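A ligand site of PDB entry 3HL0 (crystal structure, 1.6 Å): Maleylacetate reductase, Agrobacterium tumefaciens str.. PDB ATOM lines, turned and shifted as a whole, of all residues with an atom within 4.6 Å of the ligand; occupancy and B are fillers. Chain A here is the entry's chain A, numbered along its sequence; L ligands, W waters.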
ATOM      1  N   THR A  42      -8.793 -18.132  22.919  1.00  0.00           N
ATOM      2  CA  THR A  42      -8.598 -16.817  22.319  1.00  0.00           C
ATOM      3  C   THR A  42      -7.313 -16.172  22.862  1.00  0.00           C
ATOM      4  O   THR A  42      -6.685 -16.681  23.828  1.00  0.00           O
ATOM      5  CB  THR A  42      -9.760 -15.882  22.686  1.00  0.00           C
ATOM      6  OG1 THR A  42      -9.744 -15.732  24.117  1.00  0.00           O
ATOM      7  CG2 THR A  42     -11.088 -16.381  22.196  1.00  0.00           C
ATOM      8  N   GLN A  44      -7.345 -13.556  24.615  1.00  0.00           N
ATOM      9  CA  GLN A  44      -7.743 -13.021  25.919  1.00  0.00           C
ATOM     10  C   GLN A  44      -7.713 -14.060  27.034  1.00  0.00           C
ATOM     11  O   GLN A  44      -7.855 -13.716  28.229  1.00  0.00           O
ATOM     12  CB  GLN A  44      -9.132 -12.366  25.809  1.00  0.00           C
ATOM     13  CG  GLN A  44      -9.135 -11.051  24.978  1.00  0.00           C
ATOM     14  CD  GLN A  44      -9.074 -11.286  23.465  1.00  0.00           C
ATOM     15  OE1 GLN A  44      -8.290 -10.643  22.769  1.00  0.00           O
ATOM     16  NE2 GLN A  44      -9.892 -12.220  22.954  1.00  0.00           N
ATOM     17  N   GLN A  45      -7.539 -15.331  26.667  1.00  0.00           N
ATOM     18  CA  GLN A  45      -7.439 -16.404  27.651  1.00  0.00           C
ATOM     19  C   GLN A  45      -6.185 -17.281  27.422  1.00  0.00           C
ATOM     20  O   GLN A  45      -6.107 -18.410  27.926  1.00  0.00           O
ATOM     21  CB  GLN A  45      -8.710 -17.237  27.663  1.00  0.00           C
ATOM     22  CG  GLN A  45      -9.894 -16.518  28.320  1.00  0.00           C
ATOM     23  CD  GLN A  45     -11.205 -17.298  28.183  1.00  0.00           C
ATOM     24  OE1 GLN A  45     -11.840 -17.255  27.117  1.00  0.00           O
ATOM     25  NE2 GLN A  45     -11.588 -18.028  29.246  1.00  0.00           N
ATOM     26  N   HIS A  70     -16.429 -15.368  15.537  1.00  0.00           N
ATOM     27  CA  HIS A  70     -17.234 -15.813  14.387  1.00  0.00           C
ATOM     28  C   HIS A  70     -16.587 -16.970  13.624  1.00  0.00           C
ATOM     29  O   HIS A  70     -17.021 -17.269  12.503  1.00  0.00           O
ATOM     30  CB  HIS A  70     -17.548 -14.646  13.418  1.00  0.00           C
ATOM     31  CG  HIS A  70     -18.027 -13.406  14.106  1.00  0.00           C
ATOM     32  ND1 HIS A  70     -19.132 -13.393  14.929  1.00  0.00           N
ATOM     33  CD2 HIS A  70     -17.565 -12.130  14.070  1.00  0.00           C
ATOM     34  CE1 HIS A  70     -19.321 -12.163  15.384  1.00  0.00           C
ATOM     35  NE2 HIS A  70     -18.380 -11.387  14.887  1.00  0.00           N
ATOM     36  N   GLY A  96     -15.092 -19.305  25.949  1.00  0.00           N
ATOM     37  CA  GLY A  96     -16.515 -19.156  25.691  1.00  0.00           C
ATOM     38  C   GLY A  96     -16.905 -19.746  24.323  1.00  0.00           C
ATOM     39  O   GLY A  96     -16.172 -20.596  23.773  1.00  0.00           O
ATOM     40  N   GLY A  97     -18.059 -19.338  23.836  1.00  0.00           N
ATOM     41  CA  GLY A  97     -18.632 -19.828  22.594  1.00  0.00           C
ATOM     42  C   GLY A  97     -17.659 -19.699  21.430  1.00  0.00           C
ATOM     43  O   GLY A  97     -17.643 -20.565  20.586  1.00  0.00           O
ATOM     44  N   SER A  98     -16.859 -18.644  21.371  1.00  0.00           N
ATOM     45  CA  SER A  98     -15.917 -18.563  20.234  1.00  0.00           C
ATOM     46  C   SER A  98     -14.838 -19.648  20.273  1.00  0.00           C
ATOM     47  O   SER A  98     -14.418 -20.164  19.218  1.00  0.00           O
ATOM     48  CB  SER A  98     -15.290 -17.166  20.140  1.00  0.00           C
ATOM     49  OG  SER A  98     -16.315 -16.202  19.935  1.00  0.00           O
ATOM     50  N   THR A  99     -14.389 -20.022  21.461  1.00  0.00           N
ATOM     51  CA  THR A  99     -13.368 -21.063  21.589  1.00  0.00           C
ATOM     52  C   THR A  99     -14.007 -22.449  21.370  1.00  0.00           C
ATOM     53  O   THR A  99     -13.416 -23.302  20.661  1.00  0.00           O
ATOM     54  CB  THR A  99     -12.699 -20.963  22.957  1.00  0.00           C
ATOM     55  OG1 THR A  99     -12.199 -19.631  23.032  1.00  0.00           O
ATOM     56  CG2 THR A  99     -11.507 -21.948  23.053  1.00  0.00           C
ATOM     57  N   LYS A 104     -15.100 -27.120  17.668  1.00  0.00           N
ATOM     58  CA  LYS A 104     -16.101 -27.799  16.858  1.00  0.00           C
ATOM     59  C   LYS A 104     -15.686 -27.807  15.392  1.00  0.00           C
ATOM     60  O   LYS A 104     -15.860 -28.827  14.689  1.00  0.00           O
ATOM     61  CB  LYS A 104     -17.463 -27.126  17.005  1.00  0.00           C
ATOM     62  CG  LYS A 104     -18.199 -27.418  18.324  1.00  0.00           C
ATOM     63  CD  LYS A 104     -19.414 -26.499  18.461  1.00  0.00           C
ATOM     64  CE  LYS A 104     -20.417 -27.123  19.452  1.00  0.00           C
ATOM     65  NZ  LYS A 104     -21.678 -26.285  19.504  1.00  0.00           N
ATOM     66  N   THR A 119     -16.262 -21.185  29.847  1.00  0.00           N
ATOM     67  CA  THR A 119     -15.979 -20.131  30.829  1.00  0.00           C
ATOM     68  C   THR A 119     -16.967 -18.969  30.668  1.00  0.00           C
ATOM     69  O   THR A 119     -16.775 -17.925  31.268  1.00  0.00           O
ATOM     70  CB  THR A 119     -14.525 -19.632  30.716  1.00  0.00           C
ATOM     71  OG1 THR A 119     -14.304 -19.067  29.407  1.00  0.00           O
ATOM     72  CG2 THR A 119     -13.504 -20.813  30.937  1.00  0.00           C
ATOM     73  N   THR A 120     -17.992 -19.146  29.828  1.00  0.00           N
ATOM     74  CA  THR A 120     -19.108 -18.185  29.764  1.00  0.00           C
ATOM     75  C   THR A 120     -20.398 -18.954  29.890  1.00  0.00           C
ATOM     76  O   THR A 120     -20.396 -20.153  30.246  1.00  0.00           O
ATOM     77  CB  THR A 120     -19.155 -17.338  28.463  1.00  0.00           C
ATOM     78  OG1 THR A 120     -19.567 -18.154  27.348  1.00  0.00           O
ATOM     79  CG2 THR A 120     -17.779 -16.692  28.152  1.00  0.00           C
ATOM     80  N   ALA A 122     -22.690 -19.187  27.317  1.00  0.00           N
ATOM     81  CA  ALA A 122     -23.219 -19.369  25.934  1.00  0.00           C
ATOM     82  C   ALA A 122     -23.880 -20.727  25.709  1.00  0.00           C
ATOM     83  O   ALA A 122     -24.851 -20.818  24.949  1.00  0.00           O
ATOM     84  CB  ALA A 122     -22.066 -19.168  24.889  1.00  0.00           C
ATOM     85  N   SER A 124     -22.750 -23.415  24.083  1.00  0.00           N
ATOM     86  CA  SER A 124     -22.357 -24.144  22.822  1.00  0.00           C
ATOM     87  C   SER A 124     -21.808 -25.526  23.122  1.00  0.00           C
ATOM     88  O   SER A 124     -21.909 -26.451  22.262  1.00  0.00           O
ATOM     89  CB  SER A 124     -21.270 -23.345  22.139  1.00  0.00           C
ATOM     90  OG  SER A 124     -20.957 -23.901  20.851  1.00  0.00           O
ATOM     91  N   THR A 127     -24.291 -28.322  22.437  1.00  0.00           N
ATOM     92  CA  THR A 127     -25.102 -28.294  21.232  1.00  0.00           C
ATOM     93  C   THR A 127     -24.338 -28.866  20.035  1.00  0.00           C
ATOM     94  O   THR A 127     -23.103 -28.832  19.992  1.00  0.00           O
ATOM     95  CB  THR A 127     -25.579 -26.865  20.808  1.00  0.00           C
ATOM     96  OG1 THR A 127     -24.556 -26.240  20.018  1.00  0.00           O
ATOM     97  CG2 THR A 127     -25.983 -26.029  21.991  1.00  0.00           C
ATOM     98  N   ILE A 129     -24.435 -27.549  17.113  1.00  0.00           N
ATOM     99  CA  ILE A 129     -24.520 -26.466  16.120  1.00  0.00           C
ATOM    100  C   ILE A 129     -23.168 -25.768  15.948  1.00  0.00           C
ATOM    101  O   ILE A 129     -22.473 -25.524  16.946  1.00  0.00           O
ATOM    102  CB  ILE A 129     -25.565 -25.429  16.602  1.00  0.00           C
ATOM    103  CG1 ILE A 129     -26.915 -26.118  16.904  1.00  0.00           C
ATOM    104  CG2 ILE A 129     -25.760 -24.340  15.585  1.00  0.00           C
ATOM    105  CD1 ILE A 129     -27.860 -25.234  17.805  1.00  0.00           C
ATOM    106  N   LEU A 130     -22.785 -25.468  14.700  1.00  0.00           N
ATOM    107  CA  LEU A 130     -21.539 -24.733  14.457  1.00  0.00           C
ATOM    108  C   LEU A 130     -21.787 -23.592  13.456  1.00  0.00           C
ATOM    109  O   LEU A 130     -22.312 -23.843  12.374  1.00  0.00           O
ATOM    110  CB  LEU A 130     -20.468 -25.708  13.906  1.00  0.00           C
ATOM    111  CG  LEU A 130     -19.209 -25.025  13.364  1.00  0.00           C
ATOM    112  CD1 LEU A 130     -18.411 -24.267  14.454  1.00  0.00           C
ATOM    113  CD2 LEU A 130     -18.324 -26.080  12.650  1.00  0.00           C
ATOM    114  N   LEU A 157     -13.245 -21.045  37.134  1.00  0.00           N
ATOM    115  CA  LEU A 157     -12.757 -20.449  35.908  1.00  0.00           C
ATOM    116  C   LEU A 157     -13.654 -19.295  35.427  1.00  0.00           C
ATOM    117  O   LEU A 157     -13.276 -18.553  34.535  1.00  0.00           O
ATOM    118  CB  LEU A 157     -12.647 -21.502  34.819  1.00  0.00           C
ATOM    119  CG  LEU A 157     -11.758 -22.682  35.207  1.00  0.00           C
ATOM    120  CD1 LEU A 157     -11.522 -23.466  33.933  1.00  0.00           C
ATOM    121  CD2 LEU A 157     -10.446 -22.243  35.832  1.00  0.00           C
ATOM    122  N   THR A 158     -14.802 -19.159  36.063  1.00  0.00           N
ATOM    123  CA  THR A 158     -15.722 -18.060  35.757  1.00  0.00           C
ATOM    124  C   THR A 158     -15.655 -16.900  36.721  1.00  0.00           C
ATOM    125  O   THR A 158     -16.301 -15.883  36.495  1.00  0.00           O
ATOM    126  CB  THR A 158     -17.186 -18.528  35.654  1.00  0.00           C
ATOM    127  OG1 THR A 158     -17.644 -18.953  36.926  1.00  0.00           O
ATOM    128  CG2 THR A 158     -17.349 -19.619  34.580  1.00  0.00           C
ATOM    129  N   GLY A 160     -13.415 -14.884  37.055  1.00  0.00           N
ATOM    130  CA  GLY A 160     -12.787 -13.786  36.324  1.00  0.00           C
ATOM    131  C   GLY A 160     -13.567 -13.290  35.121  1.00  0.00           C
ATOM    132  O   GLY A 160     -13.070 -12.408  34.370  1.00  0.00           O
ATOM    133  N   LEU A 161     -14.777 -13.807  34.936  1.00  0.00           N
ATOM    134  CA  LEU A 161     -15.554 -13.360  33.773  1.00  0.00           C
ATOM    135  C   LEU A 161     -16.089 -11.959  34.132  1.00  0.00           C
ATOM    136  O   LEU A 161     -16.761 -11.782  35.136  1.00  0.00           O
ATOM    137  CB  LEU A 161     -16.685 -14.350  33.490  1.00  0.00           C
ATOM    138  CG  LEU A 161     -17.593 -14.048  32.278  1.00  0.00           C
ATOM    139  CD1 LEU A 161     -16.849 -14.105  30.932  1.00  0.00           C
ATOM    140  CD2 LEU A 161     -18.855 -15.029  32.293  1.00  0.00           C
ATOM    141  N   PRO A 162     -15.794 -10.949  33.296  1.00  0.00           N
ATOM    142  CA  PRO A 162     -16.185  -9.590  33.691  1.00  0.00           C
ATOM    143  C   PRO A 162     -17.697  -9.469  33.879  1.00  0.00           C
ATOM    144  O   PRO A 162     -18.481 -10.243  33.266  1.00  0.00           O
ATOM    145  CB  PRO A 162     -15.722  -8.737  32.494  1.00  0.00           C
ATOM    146  CG  PRO A 162     -14.524  -9.475  31.934  1.00  0.00           C
ATOM    147  CD  PRO A 162     -14.955 -10.956  32.084  1.00  0.00           C
ATOM    148  N   SER A 169     -24.154 -12.544  28.642  1.00  0.00           N
ATOM    149  CA  SER A 169     -24.067 -13.957  28.328  1.00  0.00           C
ATOM    150  C   SER A 169     -25.122 -14.727  29.124  1.00  0.00           C
ATOM    151  O   SER A 169     -25.705 -15.701  28.602  1.00  0.00           O
ATOM    152  CB  SER A 169     -22.649 -14.480  28.671  1.00  0.00           C
ATOM    153  OG  SER A 169     -22.500 -15.878  28.271  1.00  0.00           O
ATOM    154  N   ASN A 172     -28.226 -14.429  27.285  1.00  0.00           N
ATOM    155  CA  ASN A 172     -28.144 -15.326  26.122  1.00  0.00           C
ATOM    156  C   ASN A 172     -28.548 -16.755  26.499  1.00  0.00           C
ATOM    157  O   ASN A 172     -29.310 -17.418  25.776  1.00  0.00           O
ATOM    158  CB  ASN A 172     -26.694 -15.273  25.563  1.00  0.00           C
ATOM    159  CG  ASN A 172     -26.481 -16.081  24.266  1.00  0.00           C
ATOM    160  OD1 ASN A 172     -27.403 -16.482  23.551  1.00  0.00           O
ATOM    161  ND2 ASN A 172     -25.212 -16.285  23.974  1.00  0.00           N
ATOM    162  N   HIS A 176     -32.182 -19.247  25.328  1.00  0.00           N
ATOM    163  CA  HIS A 176     -32.299 -20.646  24.859  1.00  0.00           C
ATOM    164  C   HIS A 176     -33.460 -21.303  25.628  1.00  0.00           C
ATOM    165  O   HIS A 176     -34.299 -21.968  25.001  1.00  0.00           O
ATOM    166  CB  HIS A 176     -31.028 -21.447  25.174  1.00  0.00           C
ATOM    167  CG  HIS A 176     -29.738 -20.833  24.724  1.00  0.00           C
ATOM    168  ND1 HIS A 176     -29.573 -20.058  23.590  1.00  0.00           N
ATOM    169  CD2 HIS A 176     -28.489 -20.953  25.274  1.00  0.00           C
ATOM    170  CE1 HIS A 176     -28.304 -19.693  23.486  1.00  0.00           C
ATOM    171  NE2 HIS A 176     -27.622 -20.266  24.470  1.00  0.00           N
ATOM    172  N   LEU A 232     -31.098 -25.749  24.092  1.00  0.00           N
ATOM    173  CA  LEU A 232     -30.684 -25.228  22.763  1.00  0.00           C
ATOM    174  C   LEU A 232     -30.264 -26.386  21.858  1.00  0.00           C
ATOM    175  O   LEU A 232     -30.530 -26.377  20.625  1.00  0.00           O
ATOM    176  CB  LEU A 232     -29.512 -24.243  22.900  1.00  0.00           C
ATOM    177  CG  LEU A 232     -28.927 -23.751  21.578  1.00  0.00           C
ATOM    178  CD1 LEU A 232     -29.961 -23.022  20.678  1.00  0.00           C
ATOM    179  CD2 LEU A 232     -27.741 -22.796  21.870  1.00  0.00           C
ATOM    180  N   HIS A 255     -22.516 -10.209  19.997  1.00  0.00           N
ATOM    181  CA  HIS A 255     -23.423 -11.372  20.090  1.00  0.00           C
ATOM    182  C   HIS A 255     -24.312 -11.386  21.355  1.00  0.00           C
ATOM    183  O   HIS A 255     -25.568 -11.320  21.268  1.00  0.00           O
ATOM    184  CB  HIS A 255     -22.615 -12.671  20.030  1.00  0.00           C
ATOM    185  CG  HIS A 255     -23.427 -13.866  20.345  1.00  0.00           C
ATOM    186  ND1 HIS A 255     -24.234 -14.465  19.408  1.00  0.00           N
ATOM    187  CD2 HIS A 255     -23.596 -14.558  21.502  1.00  0.00           C
ATOM    188  CE1 HIS A 255     -24.861 -15.495  19.965  1.00  0.00           C
ATOM    189  NE2 HIS A 255     -24.468 -15.586  21.229  1.00  0.00           N
ATOM    190  N   ALA A 256     -23.677 -11.481  22.523  1.00  0.00           N
ATOM    191  CA  ALA A 256     -24.464 -11.640  23.745  1.00  0.00           C
ATOM    192  C   ALA A 256     -25.344 -10.421  23.984  1.00  0.00           C
ATOM    193  O   ALA A 256     -26.490 -10.525  24.429  1.00  0.00           O
ATOM    194  CB  ALA A 256     -23.534 -11.875  24.961  1.00  0.00           C
HETATM  195  P1  LIG L   1     -16.817 -15.258  23.331  1.00  0.00           P
HETATM  196  O1  LIG L   1     -16.462 -16.704  23.355  1.00  0.00           O
HETATM  197  O2  LIG L   1     -16.800 -14.558  22.035  1.00  0.00           O
HETATM  198  O3  LIG L   1     -15.973 -14.523  24.473  1.00  0.00           O
HETATM  199  C1  LIG L   1     -15.916 -13.096  24.471  1.00  0.00           C
HETATM  200  C2  LIG L   1     -14.614 -12.688  25.134  1.00  0.00           C
HETATM  201  O4  LIG L   1     -14.683 -13.017  26.524  1.00  0.00           O
HETATM  202  C3  LIG L   1     -13.405 -13.417  24.532  1.00  0.00           C
HETATM  203  O5  LIG L   1     -12.285 -12.536  24.336  1.00  0.00           O
HETATM  204  C4  LIG L   1     -13.097 -14.451  25.601  1.00  0.00           C
HETATM  205  O6  LIG L   1     -11.740 -14.832  25.629  1.00  0.00           O
HETATM  206  C5  LIG L   1     -13.506 -13.731  26.895  1.00  0.00           C
HETATM  207  N1  LIG L   1     -13.843 -14.667  28.003  1.00  0.00           N
HETATM  208  C6  LIG L   1     -14.706 -15.734  27.959  1.00  0.00           C
HETATM  209  N2  LIG L   1     -14.739 -16.326  29.169  1.00  0.00           N
HETATM  210  C7  LIG L   1     -13.885 -15.657  30.013  1.00  0.00           C
HETATM  211  C8  LIG L   1     -13.534 -15.850  31.340  1.00  0.00           C
HETATM  212  N3  LIG L   1     -14.227 -16.636  32.214  1.00  0.00           N
HETATM  213  N4  LIG L   1     -12.601 -14.952  31.870  1.00  0.00           N
HETATM  214  C9  LIG L   1     -12.080 -13.930  31.117  1.00  0.00           C
HETATM  215  N5  LIG L   1     -12.437 -13.734  29.806  1.00  0.00           N
HETATM  216  C10 LIG L   1     -13.328 -14.608  29.263  1.00  0.00           C
HETATM  217  O7  LIG L   1     -18.337 -15.009  23.870  1.00  0.00           O
HETATM  218  P2  LIG L   1     -19.604 -16.020  23.957  1.00  0.00           P
HETATM  219  O8  LIG L   1     -20.783 -15.124  24.105  1.00  0.00           O
HETATM  220  O9  LIG L   1     -19.262 -17.000  24.986  1.00  0.00           O
HETATM  221  O10 LIG L   1     -19.706 -16.734  22.524  1.00  0.00           O
HETATM  222  C11 LIG L   1     -20.239 -16.078  21.383  1.00  0.00           C
HETATM  223  C12 LIG L   1     -19.977 -16.981  20.176  1.00  0.00           C
HETATM  224  O11 LIG L   1     -20.494 -18.262  20.461  1.00  0.00           O
HETATM  225  C13 LIG L   1     -20.728 -16.464  18.956  1.00  0.00           C
HETATM  226  O12 LIG L   1     -19.946 -16.775  17.798  1.00  0.00           O
HETATM  227  C14 LIG L   1     -22.005 -17.271  18.986  1.00  0.00           C
HETATM  228  O13 LIG L   1     -22.667 -17.388  17.731  1.00  0.00           O
HETATM  229  C15 LIG L   1     -21.490 -18.602  19.502  1.00  0.00           C
HETATM  230  N6  LIG L   1     -22.515 -19.428  20.119  1.00  0.00           N
HETATM  231  C16 LIG L   1     -22.754 -20.648  19.556  1.00  0.00           C
HETATM  232  C17 LIG L   1     -23.713 -21.467  20.109  1.00  0.00           C
HETATM  233  C18 LIG L   1     -23.859 -22.763  19.431  1.00  0.00           C
HETATM  234  O14 LIG L   1     -24.734 -23.593  20.024  1.00  0.00           O
HETATM  235  N7  LIG L   1     -23.162 -23.071  18.315  1.00  0.00           N
HETATM  236  C19 LIG L   1     -24.449 -21.108  21.289  1.00  0.00           C
HETATM  237  C20 LIG L   1     -24.195 -19.856  21.846  1.00  0.00           C
HETATM  238  C21 LIG L   1     -23.234 -19.019  21.247  1.00  0.00           C
HETATM  239  O   HOH W   1     -18.590 -12.621  21.366  1.00  0.00           O
HETATM  240  O   HOH W   2     -20.800 -12.497  23.032  1.00  0.00           O
HETATM  241  O   HOH W   3     -11.139 -15.508  33.966  1.00  0.00           O
HETATM  242  O   HOH W   4     -27.008 -18.149  20.747  1.00  0.00           O
HETATM  243  O   HOH W   5     -22.989 -15.740  25.576  1.00  0.00           O
HETATM  244  O   HOH W   6     -14.712 -10.985  28.432  1.00  0.00           O
HETATM  245  O   HOH W   7     -17.741 -15.188  17.934  1.00  0.00           O
HETATM  246  O   HOH W   8     -13.977 -17.584  24.043  1.00  0.00           O
HETATM  247  O   HOH W   9     -20.634 -21.711  16.749  1.00  0.00           O
HETATM  248  O   HOH W  10     -12.199 -10.791  29.090  1.00  0.00           O
HETATM  249  O   HOH W  11     -19.660 -22.228  19.491  1.00  0.00           O
HETATM  250  O   HOH W  12     -15.442 -12.579  19.691  1.00  0.00           O
HETATM  251  O   HOH W  13     -11.776 -10.283  26.280  1.00  0.00           O
HETATM  252  O   HOH W  14     -25.154 -18.120  17.883  1.00  0.00           O
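Gly 96 touches the ligand (C to O1, 3.2 Å). NZ of Lys 104 touches N7 of the ligand, 3.7 Å away. Ala 122 touches the ligand. Gly 160 touches the ligand (O to N4, 3.6 Å). Leu 161 touches the ligand (CD1 to C7, 3.5 Å). CD2 of Leu 232 touches O14 of the ligand, 3.6 Å away. His 255 touches the ligand. 18 residues have an atom within 4 Å of the ligand: Thr 42, Gln 44, Gln 45, Gly 96, Gly 97, Ser 98, Lys 104, Thr 119, Thr 120, Ala 122, Ser 124, Thr 127, Ile 129, Leu 157, Gly 160, Leu 161, Leu 232 and His 255. Along chain A the residues within 4 Å of the ligand span positions 42 to 255. The nearest printed residue that does not touch the ligand is Thr 158 (4.1 Å).
Water W7 lies within hydrogen-bond range of OG of Ser 98 (2.7 Å), O12 of the ligand (2.7 Å) and N of His 70 (2.7 Å). Water W5 lies within hydrogen-bond range of O8 of the ligand, OG of Ser 169 and ND2 of Asn 172. Water W8 lies within hydrogen-bond range of O1 of the ligand, N of Gly 96 and OG1 of Thr 99. Water W2 lies within hydrogen-bond range of O8 of the ligand (2.8 Å) and N of Ala 256 (3.1 Å). Water W11 bridges OG of Ser 124 (2.5 Å) and O of Gly 97 (2.8 Å).
N of Ile 129 sits at hydrogen-bond distance from OG1 of Thr 127, 3.2 Å away. The side-chain hydroxyl of Thr 127 lies within hydrogen-bond range of the backbone carbonyl oxygen of Ser 124 (3.5 Å). The side-chain hydroxyl of Thr 42 sits close to the backbone NH of Gln 44 (3.3 Å). N of Gln 45 is in hydrogen-bond range of OG1 of Thr 42. The side-chain hydroxyl (OG1) of Thr 119 sits at hydrogen-bond distance from the side-chain amide nitrogen (NE2) of Gln 45. The backbone carbonyl oxygen (O) of Ile 129 sits at hydrogen-bond distance from the side-chain amino group (NZ) of Lys 104. The backbone carbonyl oxygen (O) of Ala 122 is in hydrogen-bond range of a ring nitrogen (NE2) of His 176. The backbone NH (N) of Ala 122 sits at hydrogen-bond distance from the side-chain hydroxyl (OG) of Ser 169, at 3.4 Å.
The side-chain hydroxyl of Thr 120 lies within hydrogen-bond range of an oxygen (O9) of the ligand. An oxygen (O14) of the ligand lies within hydrogen-bond range of the side-chain hydroxyl of Thr 127 (2.7 Å). The side-chain hydroxyl (OG1) of Thr 42 lies within hydrogen-bond range of an oxygen (O6) of the ligand, at 2.7 Å. An oxygen (O1) of the ligand lies within hydrogen-bond range of the backbone NH (N) of Ser 98, at 2.8 Å. An oxygen (O2) of the ligand sits at hydrogen-bond distance from the side-chain hydroxyl of Ser 98 (2.7 Å). An oxygen (O5) of the ligand is in hydrogen-bond range of the side-chain amide nitrogen of Gln 44 (2.8 Å). A nitrogen (N3) of the ligand sits at hydrogen-bond distance from the backbone carbonyl oxygen (O) of Thr 119 (3.0 Å). The side-chain hydroxyl (OG1) of Thr 119 sits at hydrogen-bond distance from a nitrogen (N2) of the ligand, 2.8 Å away. O6 of the ligand is in hydrogen-bond range of OE1 of Gln 45 (2.8 Å). The backbone NH (N) of Gly 97 sits at hydrogen-bond distance from an oxygen (O9) of the ligand, 2.9 Å away. A nitrogen (N7) of the ligand lies within hydrogen-bond range of the backbone carbonyl oxygen of Ile 129 (2.9 Å). A nitrogen (N3) of the ligand is in hydrogen-bond range of the backbone carbonyl oxygen of Leu 157, at 3.2 Å. A nitrogen (N7) of the ligand lies close to the side-chain hydroxyl (OG) of Ser 124 (3.5 Å).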
